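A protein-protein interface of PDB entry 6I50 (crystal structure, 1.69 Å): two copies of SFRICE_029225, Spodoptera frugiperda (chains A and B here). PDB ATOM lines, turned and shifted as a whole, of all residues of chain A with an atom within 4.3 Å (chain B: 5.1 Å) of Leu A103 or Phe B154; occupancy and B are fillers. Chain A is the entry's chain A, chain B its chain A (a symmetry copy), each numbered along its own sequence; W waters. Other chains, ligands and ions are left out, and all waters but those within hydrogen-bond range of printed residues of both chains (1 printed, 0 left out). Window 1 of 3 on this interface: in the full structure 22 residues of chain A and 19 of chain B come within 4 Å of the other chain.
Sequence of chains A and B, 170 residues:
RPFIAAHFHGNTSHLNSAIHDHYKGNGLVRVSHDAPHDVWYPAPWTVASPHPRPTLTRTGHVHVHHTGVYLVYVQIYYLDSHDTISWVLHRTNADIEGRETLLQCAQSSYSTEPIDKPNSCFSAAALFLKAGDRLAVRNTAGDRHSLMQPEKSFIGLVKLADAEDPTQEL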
ATOM      1  N   TRP A  87     -16.614   8.856 -16.345  1.00  0.00           N
ATOM      2  CA  TRP A  87     -16.657  10.089 -15.572  1.00  0.00           C
ATOM      3  C   TRP A  87     -15.297  10.379 -14.952  1.00  0.00           C
ATOM      4  O   TRP A  87     -14.447   9.490 -14.795  1.00  0.00           O
ATOM      5  CB  TRP A  87     -17.744  10.055 -14.476  1.00  0.00           C
ATOM      6  CG  TRP A  87     -17.654   8.945 -13.458  1.00  0.00           C
ATOM      7  CD1 TRP A  87     -18.443   7.833 -13.393  1.00  0.00           C
ATOM      8  CD2 TRP A  87     -16.772   8.879 -12.328  1.00  0.00           C
ATOM      9  NE1 TRP A  87     -18.099   7.066 -12.300  1.00  0.00           N
ATOM     10  CE2 TRP A  87     -17.072   7.684 -11.632  1.00  0.00           C
ATOM     11  CE3 TRP A  87     -15.753   9.705 -11.843  1.00  0.00           C
ATOM     12  CZ2 TRP A  87     -16.383   7.295 -10.484  1.00  0.00           C
ATOM     13  CZ3 TRP A  87     -15.069   9.316 -10.703  1.00  0.00           C
ATOM     14  CH2 TRP A  87     -15.385   8.119 -10.038  1.00  0.00           C
ATOM     15  N   VAL A  88     -15.105  11.654 -14.606  1.00  0.00           N
ATOM     16  CA  VAL A  88     -13.916  12.127 -13.906  1.00  0.00           C
ATOM     17  C   VAL A  88     -14.355  12.933 -12.692  1.00  0.00           C
ATOM     18  O   VAL A  88     -15.374  13.631 -12.728  1.00  0.00           O
ATOM     19  CB  VAL A  88     -12.997  12.977 -14.811  1.00  0.00           C
ATOM     20  CG1 VAL A  88     -12.226  12.076 -15.771  1.00  0.00           C
ATOM     21  CG2 VAL A  88     -13.803  14.010 -15.569  1.00  0.00           C
ATOM     22  N   LEU A  89     -13.584  12.825 -11.613  1.00  0.00           N
ATOM     23  CA  LEU A  89     -13.799  13.613 -10.409  1.00  0.00           C
ATOM     24  C   LEU A  89     -12.844  14.801 -10.456  1.00  0.00           C
ATOM     25  O   LEU A  89     -11.628  14.611 -10.438  1.00  0.00           O
ATOM     26  CB  LEU A  89     -13.547  12.757  -9.166  1.00  0.00           C
ATOM     27  CG  LEU A  89     -13.700  13.494  -7.838  1.00  0.00           C
ATOM     28  CD1 LEU A  89     -15.146  13.923  -7.632  1.00  0.00           C
ATOM     29  CD2 LEU A  89     -13.227  12.643  -6.668  1.00  0.00           C
ATOM     30  N   THR A 101      -7.833  16.311 -11.885  1.00  0.00           N
ATOM     31  CA  THR A 101      -8.589  15.069 -11.993  1.00  0.00           C
ATOM     32  C   THR A 101      -8.042  14.080 -10.968  1.00  0.00           C
ATOM     33  O   THR A 101      -6.879  13.673 -11.056  1.00  0.00           O
ATOM     34  CB  THR A 101      -8.490  14.494 -13.407  1.00  0.00           C
ATOM     35  OG1 THR A 101      -8.979  15.456 -14.358  1.00  0.00           O
ATOM     36  CG2 THR A 101      -9.304  13.221 -13.512  1.00  0.00           C
ATOM     37  N   LEU A 102      -8.872  13.707  -9.994  1.00  0.00           N
ATOM     38  CA  LEU A 102      -8.440  12.839  -8.906  1.00  0.00           C
ATOM     39  C   LEU A 102      -8.788  11.382  -9.138  1.00  0.00           C
ATOM     40  O   LEU A 102      -8.074  10.501  -8.652  1.00  0.00           O
ATOM     41  CB  LEU A 102      -9.072  13.282  -7.581  1.00  0.00           C
ATOM     42  CG  LEU A 102      -8.765  14.717  -7.151  1.00  0.00           C
ATOM     43  CD1 LEU A 102      -9.238  14.935  -5.724  1.00  0.00           C
ATOM     44  CD2 LEU A 102      -7.277  15.002  -7.280  1.00  0.00           C
ATOM     45  N   LEU A 103      -9.869  11.121  -9.871  1.00  0.00           N
ATOM     46  CA  LEU A 103     -10.420   9.781 -10.019  1.00  0.00           C
ATOM     47  C   LEU A 103     -11.111   9.693 -11.369  1.00  0.00           C
ATOM     48  O   LEU A 103     -11.684  10.673 -11.847  1.00  0.00           O
ATOM     49  CB  LEU A 103     -11.412   9.484  -8.887  1.00  0.00           C
ATOM     50  CG  LEU A 103     -11.620   8.101  -8.300  1.00  0.00           C
ATOM     51  CD1 LEU A 103     -10.290   7.477  -7.903  1.00  0.00           C
ATOM     52  CD2 LEU A 103     -12.536   8.248  -7.088  1.00  0.00           C
ATOM     53  N   GLN A 104     -11.054   8.512 -11.984  1.00  0.00           N
ATOM     54  CA  GLN A 104     -11.732   8.294 -13.253  1.00  0.00           C
ATOM     55  C   GLN A 104     -12.261   6.869 -13.307  1.00  0.00           C
ATOM     56  O   GLN A 104     -11.629   5.943 -12.793  1.00  0.00           O
ATOM     57  CB  GLN A 104     -10.806   8.551 -14.445  1.00  0.00           C
ATOM     58  CG  GLN A 104     -11.504   8.433 -15.800  1.00  0.00           C
ATOM     59  CD  GLN A 104     -10.683   9.002 -16.937  1.00  0.00           C
ATOM     60  OE1 GLN A 104      -9.584   9.508 -16.730  1.00  0.00           O
ATOM     61  NE2 GLN A 104     -11.217   8.923 -18.148  1.00  0.00           N
ATOM     62  N   SER A 123     -16.122   4.089  -8.516  1.00  0.00           N
ATOM     63  CA  SER A 123     -14.726   4.096  -8.093  1.00  0.00           C
ATOM     64  C   SER A 123     -14.615   4.771  -6.735  1.00  0.00           C
ATOM     65  O   SER A 123     -15.504   5.516  -6.312  1.00  0.00           O
ATOM     66  CB  SER A 123     -13.809   4.790  -9.113  1.00  0.00           C
ATOM     67  OG  SER A 123     -12.441   4.488  -8.841  1.00  0.00           O
ATOM     68  N   ALA A 124     -13.503   4.501  -6.055  1.00  0.00           N
ATOM     69  CA  ALA A 124     -13.269   5.046  -4.726  1.00  0.00           C
ATOM     70  C   ALA A 124     -11.777   5.026  -4.446  1.00  0.00           C
ATOM     71  O   ALA A 124     -11.035   4.236  -5.032  1.00  0.00           O
ATOM     72  CB  ALA A 124     -14.030   4.256  -3.652  1.00  0.00           C
ATOM     73  N   ALA A 125     -11.345   5.910  -3.547  1.00  0.00           N
ATOM     74  CA  ALA A 125      -9.939   5.937  -3.151  1.00  0.00           C
ATOM     75  C   ALA A 125      -9.777   6.815  -1.921  1.00  0.00           C
ATOM     76  O   ALA A 125     -10.633   7.648  -1.615  1.00  0.00           O
ATOM     77  CB  ALA A 125      -9.039   6.451  -4.280  1.00  0.00           C
ATOM     78  N   HIS B   7      -1.757   4.705  -0.021  1.00  0.00           N
ATOM     79  CA  HIS B   7      -2.363   4.687  -1.344  1.00  0.00           C
ATOM     80  C   HIS B   7      -1.247   4.753  -2.372  1.00  0.00           C
ATOM     81  O   HIS B   7      -0.382   5.625  -2.286  1.00  0.00           O
ATOM     82  CB  HIS B   7      -3.325   5.862  -1.540  1.00  0.00           C
ATOM     83  CG  HIS B   7      -3.983   5.885  -2.883  1.00  0.00           C
ATOM     84  ND1 HIS B   7      -5.152   5.203  -3.151  1.00  0.00           N
ATOM     85  CD2 HIS B   7      -3.634   6.499  -4.038  1.00  0.00           C
ATOM     86  CE1 HIS B   7      -5.501   5.411  -4.409  1.00  0.00           C
ATOM     87  NE2 HIS B   7      -4.598   6.197  -4.968  1.00  0.00           N
ATOM     88  N   PHE B   8      -1.245   3.815  -3.314  1.00  0.00           N
ATOM     89  CA  PHE B   8      -0.252   3.766  -4.381  1.00  0.00           C
ATOM     90  C   PHE B   8      -0.984   3.829  -5.711  1.00  0.00           C
ATOM     91  O   PHE B   8      -1.967   3.107  -5.912  1.00  0.00           O
ATOM     92  CB  PHE B   8       0.586   2.487  -4.295  1.00  0.00           C
ATOM     93  CG  PHE B   8       1.133   2.224  -2.927  1.00  0.00           C
ATOM     94  CD1 PHE B   8       2.307   2.832  -2.515  1.00  0.00           C
ATOM     95  CD2 PHE B   8       0.457   1.397  -2.040  1.00  0.00           C
ATOM     96  CE1 PHE B   8       2.816   2.604  -1.247  1.00  0.00           C
ATOM     97  CE2 PHE B   8       0.960   1.158  -0.771  1.00  0.00           C
ATOM     98  CZ  PHE B   8       2.141   1.774  -0.374  1.00  0.00           C
ATOM     99  N   HIS B   9      -0.516   4.676  -6.623  1.00  0.00           N
ATOM    100  CA  HIS B   9      -1.233   4.840  -7.879  1.00  0.00           C
ATOM    101  C   HIS B   9      -0.284   4.700  -9.061  1.00  0.00           C
ATOM    102  O   HIS B   9       0.942   4.722  -8.917  1.00  0.00           O
ATOM    103  CB  HIS B   9      -1.999   6.183  -7.937  1.00  0.00           C
ATOM    104  CG  HIS B   9      -1.154   7.395  -7.691  1.00  0.00           C
ATOM    105  ND1 HIS B   9      -1.637   8.509  -7.038  1.00  0.00           N
ATOM    106  CD2 HIS B   9       0.121   7.689  -8.041  1.00  0.00           C
ATOM    107  CE1 HIS B   9      -0.692   9.429  -6.978  1.00  0.00           C
ATOM    108  NE2 HIS B   9       0.386   8.958  -7.580  1.00  0.00           N
ATOM    109  N   GLY B  10      -0.875   4.517 -10.239  1.00  0.00           N
ATOM    110  CA  GLY B  10      -0.075   4.307 -11.433  1.00  0.00           C
ATOM    111  C   GLY B  10       0.724   5.552 -11.775  1.00  0.00           C
ATOM    112  O   GLY B  10       0.212   6.671 -11.742  1.00  0.00           O
ATOM    113  N   TRP B  40       3.612   1.203  -9.802  1.00  0.00           N
ATOM    114  CA  TRP B  40       2.977   1.901  -8.694  1.00  0.00           C
ATOM    115  C   TRP B  40       3.924   2.934  -8.099  1.00  0.00           C
ATOM    116  O   TRP B  40       5.148   2.815  -8.187  1.00  0.00           O
ATOM    117  CB  TRP B  40       2.571   0.932  -7.576  1.00  0.00           C
ATOM    118  CG  TRP B  40       1.637  -0.173  -7.941  1.00  0.00           C
ATOM    119  CD1 TRP B  40       1.814  -1.505  -7.699  1.00  0.00           C
ATOM    120  CD2 TRP B  40       0.357  -0.047  -8.573  1.00  0.00           C
ATOM    121  NE1 TRP B  40       0.728  -2.217  -8.151  1.00  0.00           N
ATOM    122  CE2 TRP B  40      -0.181  -1.346  -8.688  1.00  0.00           C
ATOM    123  CE3 TRP B  40      -0.386   1.035  -9.054  1.00  0.00           C
ATOM    124  CZ2 TRP B  40      -1.423  -1.591  -9.268  1.00  0.00           C
ATOM    125  CZ3 TRP B  40      -1.615   0.788  -9.632  1.00  0.00           C
ATOM    126  CH2 TRP B  40      -2.120  -0.510  -9.737  1.00  0.00           C
ATOM    127  N   TYR B  73      -8.492  -1.787  -1.455  1.00  0.00           N
ATOM    128  CA  TYR B  73      -9.191  -1.494  -2.700  1.00  0.00           C
ATOM    129  C   TYR B  73      -8.188  -1.447  -3.844  1.00  0.00           C
ATOM    130  O   TYR B  73      -7.024  -1.072  -3.660  1.00  0.00           O
ATOM    131  CB  TYR B  73      -9.991  -0.178  -2.608  1.00  0.00           C
ATOM    132  CG  TYR B  73      -9.154   1.029  -2.251  1.00  0.00           C
ATOM    133  CD1 TYR B  73      -8.468   1.736  -3.239  1.00  0.00           C
ATOM    134  CD2 TYR B  73      -9.046   1.461  -0.931  1.00  0.00           C
ATOM    135  CE1 TYR B  73      -7.683   2.831  -2.916  1.00  0.00           C
ATOM    136  CE2 TYR B  73      -8.268   2.566  -0.600  1.00  0.00           C
ATOM    137  CZ  TYR B  73      -7.592   3.244  -1.599  1.00  0.00           C
ATOM    138  OH  TYR B  73      -6.818   4.331  -1.275  1.00  0.00           O
ATOM    139  N   VAL B  74      -8.644  -1.861  -5.022  1.00  0.00           N
ATOM    140  CA  VAL B  74      -7.808  -1.942  -6.214  1.00  0.00           C
ATOM    141  C   VAL B  74      -8.626  -1.492  -7.413  1.00  0.00           C
ATOM    142  O   VAL B  74      -9.792  -1.875  -7.559  1.00  0.00           O
ATOM    143  CB  VAL B  74      -7.284  -3.376  -6.446  1.00  0.00           C
ATOM    144  CG1 VAL B  74      -6.552  -3.477  -7.778  1.00  0.00           C
ATOM    145  CG2 VAL B  74      -6.391  -3.836  -5.296  1.00  0.00           C
ATOM    146  N   GLN B  75      -8.009  -0.697  -8.287  1.00  0.00           N
ATOM    147  CA  GLN B  75      -8.583  -0.403  -9.595  1.00  0.00           C
ATOM    148  C   GLN B  75      -7.509  -0.546 -10.663  1.00  0.00           C
ATOM    149  O   GLN B  75      -6.431   0.049 -10.550  1.00  0.00           O
ATOM    150  CB  GLN B  75      -9.179   1.002  -9.657  1.00  0.00           C
ATOM    151  CG  GLN B  75      -9.747   1.341 -11.034  1.00  0.00           C
ATOM    152  CD  GLN B  75     -10.664   2.542 -10.990  1.00  0.00           C
ATOM    153  OE1 GLN B  75     -11.709   2.510 -10.339  1.00  0.00           O
ATOM    154  NE2 GLN B  75     -10.285   3.610 -11.694  1.00  0.00           N
ATOM    155  N   PHE B 122     -12.782  -2.286 -10.640  1.00  0.00           N
ATOM    156  CA  PHE B 122     -12.600  -1.906  -9.244  1.00  0.00           C
ATOM    157  C   PHE B 122     -13.174  -2.979  -8.326  1.00  0.00           C
ATOM    158  O   PHE B 122     -14.251  -3.524  -8.591  1.00  0.00           O
ATOM    159  CB  PHE B 122     -13.283  -0.559  -8.951  1.00  0.00           C
ATOM    160  CG  PHE B 122     -13.198  -0.135  -7.511  1.00  0.00           C
ATOM    161  CD1 PHE B 122     -14.070  -0.655  -6.552  1.00  0.00           C
ATOM    162  CD2 PHE B 122     -12.248   0.794  -7.115  1.00  0.00           C
ATOM    163  CE1 PHE B 122     -13.967  -0.282  -5.228  1.00  0.00           C
ATOM    164  CE2 PHE B 122     -12.143   1.182  -5.793  1.00  0.00           C
ATOM    165  CZ  PHE B 122     -13.005   0.643  -4.844  1.00  0.00           C
ATOM    166  N   PRO B 150      -2.370   8.176 -12.424  1.00  0.00           N
ATOM    167  CA  PRO B 150      -2.744   8.144 -10.999  1.00  0.00           C
ATOM    168  C   PRO B 150      -4.238   8.083 -10.764  1.00  0.00           C
ATOM    169  O   PRO B 150      -4.693   7.405  -9.836  1.00  0.00           O
ATOM    170  CB  PRO B 150      -2.141   9.447 -10.453  1.00  0.00           C
ATOM    171  CG  PRO B 150      -1.093   9.829 -11.425  1.00  0.00           C
ATOM    172  CD  PRO B 150      -1.575   9.369 -12.762  1.00  0.00           C
ATOM    173  N   GLU B 151      -5.019   8.788 -11.575  1.00  0.00           N
ATOM    174  CA  GLU B 151      -6.463   8.786 -11.406  1.00  0.00           C
ATOM    175  C   GLU B 151      -7.124   7.524 -11.952  1.00  0.00           C
ATOM    176  O   GLU B 151      -8.304   7.296 -11.665  1.00  0.00           O
ATOM    177  CB  GLU B 151      -7.057  10.027 -12.079  1.00  0.00           C
ATOM    178  CG  GLU B 151      -7.160   9.949 -13.607  1.00  0.00           C
ATOM    179  CD  GLU B 151      -5.864  10.258 -14.332  1.00  0.00           C
ATOM    180  OE1 GLU B 151      -4.814  10.461 -13.678  1.00  0.00           O
ATOM    181  OE2 GLU B 151      -5.902  10.307 -15.580  1.00  0.00           O
ATOM    182  N   LYS B 152      -6.400   6.699 -12.708  1.00  0.00           N
ATOM    183  CA  LYS B 152      -6.998   5.559 -13.399  1.00  0.00           C
ATOM    184  C   LYS B 152      -6.728   4.217 -12.723  1.00  0.00           C
ATOM    185  O   LYS B 152      -7.622   3.367 -12.672  1.00  0.00           O
ATOM    186  CB  LYS B 152      -6.500   5.512 -14.851  1.00  0.00           C
ATOM    187  CG  LYS B 152      -7.028   6.661 -15.707  1.00  0.00           C
ATOM    188  CD  LYS B 152      -6.815   6.401 -17.193  1.00  0.00           C
ATOM    189  CE  LYS B 152      -7.512   7.459 -18.042  1.00  0.00           C
ATOM    190  NZ  LYS B 152      -6.847   8.795 -17.940  1.00  0.00           N
ATOM    191  N   SER B 153      -5.521   3.991 -12.207  1.00  0.00           N
ATOM    192  CA  SER B 153      -5.143   2.694 -11.652  1.00  0.00           C
ATOM    193  C   SER B 153      -4.441   2.895 -10.318  1.00  0.00           C
ATOM    194  O   SER B 153      -3.596   3.787 -10.192  1.00  0.00           O
ATOM    195  CB  SER B 153      -4.229   1.913 -12.612  1.00  0.00           C
ATOM    196  OG  SER B 153      -4.892   1.630 -13.838  1.00  0.00           O
ATOM    197  N   PHE B 154      -4.788   2.073  -9.323  1.00  0.00           N
ATOM    198  CA  PHE B 154      -4.248   2.290  -7.983  1.00  0.00           C
ATOM    199  C   PHE B 154      -4.546   1.089  -7.093  1.00  0.00           C
ATOM    200  O   PHE B 154      -5.381   0.238  -7.412  1.00  0.00           O
ATOM    201  CB  PHE B 154      -4.821   3.565  -7.355  1.00  0.00           C
ATOM    202  CG  PHE B 154      -6.316   3.713  -7.523  1.00  0.00           C
ATOM    203  CD1 PHE B 154      -7.192   3.064  -6.666  1.00  0.00           C
ATOM    204  CD2 PHE B 154      -6.838   4.513  -8.527  1.00  0.00           C
ATOM    205  CE1 PHE B 154      -8.562   3.198  -6.818  1.00  0.00           C
ATOM    206  CE2 PHE B 154      -8.207   4.653  -8.683  1.00  0.00           C
ATOM    207  CZ  PHE B 154      -9.071   4.001  -7.819  1.00  0.00           C
ATOM    208  N   ILE B 155      -3.859   1.050  -5.951  1.00  0.00           N
ATOM    209  CA  ILE B 155      -4.111   0.078  -4.890  1.00  0.00           C
ATOM    210  C   ILE B 155      -3.870   0.779  -3.560  1.00  0.00           C
ATOM    211  O   ILE B 155      -2.878   1.494  -3.395  1.00  0.00           O
ATOM    212  CB  ILE B 155      -3.231  -1.186  -5.018  1.00  0.00           C
ATOM    213  CG1 ILE B 155      -3.395  -2.089  -3.791  1.00  0.00           C
ATOM    214  CG2 ILE B 155      -1.756  -0.831  -5.217  1.00  0.00           C
ATOM    215  CD1 ILE B 155      -2.756  -3.461  -3.947  1.00  0.00           C
ATOM    216  N   GLY B 156      -4.813   0.633  -2.634  1.00  0.00           N
ATOM    217  CA  GLY B 156      -4.709   1.301  -1.355  1.00  0.00           C
ATOM    218  C   GLY B 156      -5.271   0.424  -0.258  1.00  0.00           C
ATOM    219  O   GLY B 156      -6.009  -0.535  -0.510  1.00  0.00           O
HETATM  220  O   HOH W   1      -8.228  11.760 -16.983  1.00  0.00           O
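Of chain B, only Glu B151 and Phe B154 come within 4 Å of Leu A103. Of chain A, only Leu A103, Ser A123 and Ala A124 come within 4 Å of Phe B154. Of the printed residues of chain B, Thr A101 touches Glu B151. Of the printed residues of chain A, Gln B75 touches Gln A104 and Ser A123. Of the printed residues of chain A, Lys B152 touches Gln A104. Of the printed residues of chain B, Leu A102 touches Glu B151 (3.6 Å). Printed residues of chain B within 4 Å of Ala A124: Phe B122 (3.3 Å) and Phe B154 (3.2 Å). The nearest printed residue of chain B that does not touch Leu A103 is Gln B75 (5.4 Å). The nearest residue of chain A that does not touch Phe B154 is Ala A125 (4.2 Å). The nearest printed residue of chain A that does not touch Lys B152 is Leu A103 (5.7 Å).
Water W1 lies within hydrogen-bond range of the side-chain amide oxygen of Gln A104, the side-chain carboxylate of Glu B151 and the side-chain amino group of Lys B152.
The backbone carbonyl oxygen (O) of Glu B151 is in hydrogen-bond range of the backbone NH (N) of Gln A104, 3.0 Å away. The side-chain amino group of Lys B152 sits at hydrogen-bond distance from the side-chain amide oxygen of Gln A104 (3.1 Å). OG of Ser A123 lies within hydrogen-bond range of OE1 of Gln B75 (2.6 Å). The side-chain amide nitrogen (NE2) of Gln B75 lies within hydrogen-bond range of the backbone carbonyl oxygen (O) of Gln A104 (2.9 Å).
Among the printed residues, merely in contact across the chains: Ala A124 with Phe B154, Ala A124 with Phe B122, Ser A123 with Phe B154, Leu A103 with Phe B154, Leu A102 with Glu B151, Leu A103 with Glu B151, Ala A125 with His B7, Thr A101 with Glu B151 and Ala A125 with Tyr B73.
The backbone carbonyl oxygen (O) of Gly B156 lies within hydrogen-bond range of the backbone NH (N) of Tyr B73, at 2.9 Å. The backbone carbonyl oxygen (O) of Lys B152 lies within hydrogen-bond range of the side-chain amide nitrogen (NE2) of Gln B75 (2.8 Å). A ring nitrogen (ND1) of His B7 is in hydrogen-bond range of the side-chain hydroxyl (OH) of Tyr B73, at 2.7 Å. N of Leu A89 sits at hydrogen-bond distance from O of Leu A103. The backbone carbonyl oxygen of Gln B75 is in hydrogen-bond range of the backbone NH of Phe B154, at 2.9 Å. The backbone carbonyl oxygen (O) of Leu A89 sits at hydrogen-bond distance from the backbone NH (N) of Leu A102 (2.9 Å).
Of the 16 printed residues of chain B, 7 touch a printed residue of chain A. Printed residues of chain B that touch a printed residue of chain A: His B7, Tyr B73, Gln B75, Phe B122, Glu B151, Lys B152 and Phe B154. Hydrophobic or aromatic side chains of chain B within 4 Å of the printed part of chain A: His B7, Tyr B73, Phe B122 and Phe B154. Of the 10 printed residues of chain A, 7 touch a printed residue of chain B. Hydrophobic or aromatic side chains of chain A that line the printed part of chain B: Leu A103, Ala A124 and Ala A125. Among the printed residues, 13 pairs touch across the chains.
No position is printed for both chains. Of the 13 pairs that touch across the chains among the printed residues, none has its exchanged pair printed and touching as well.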
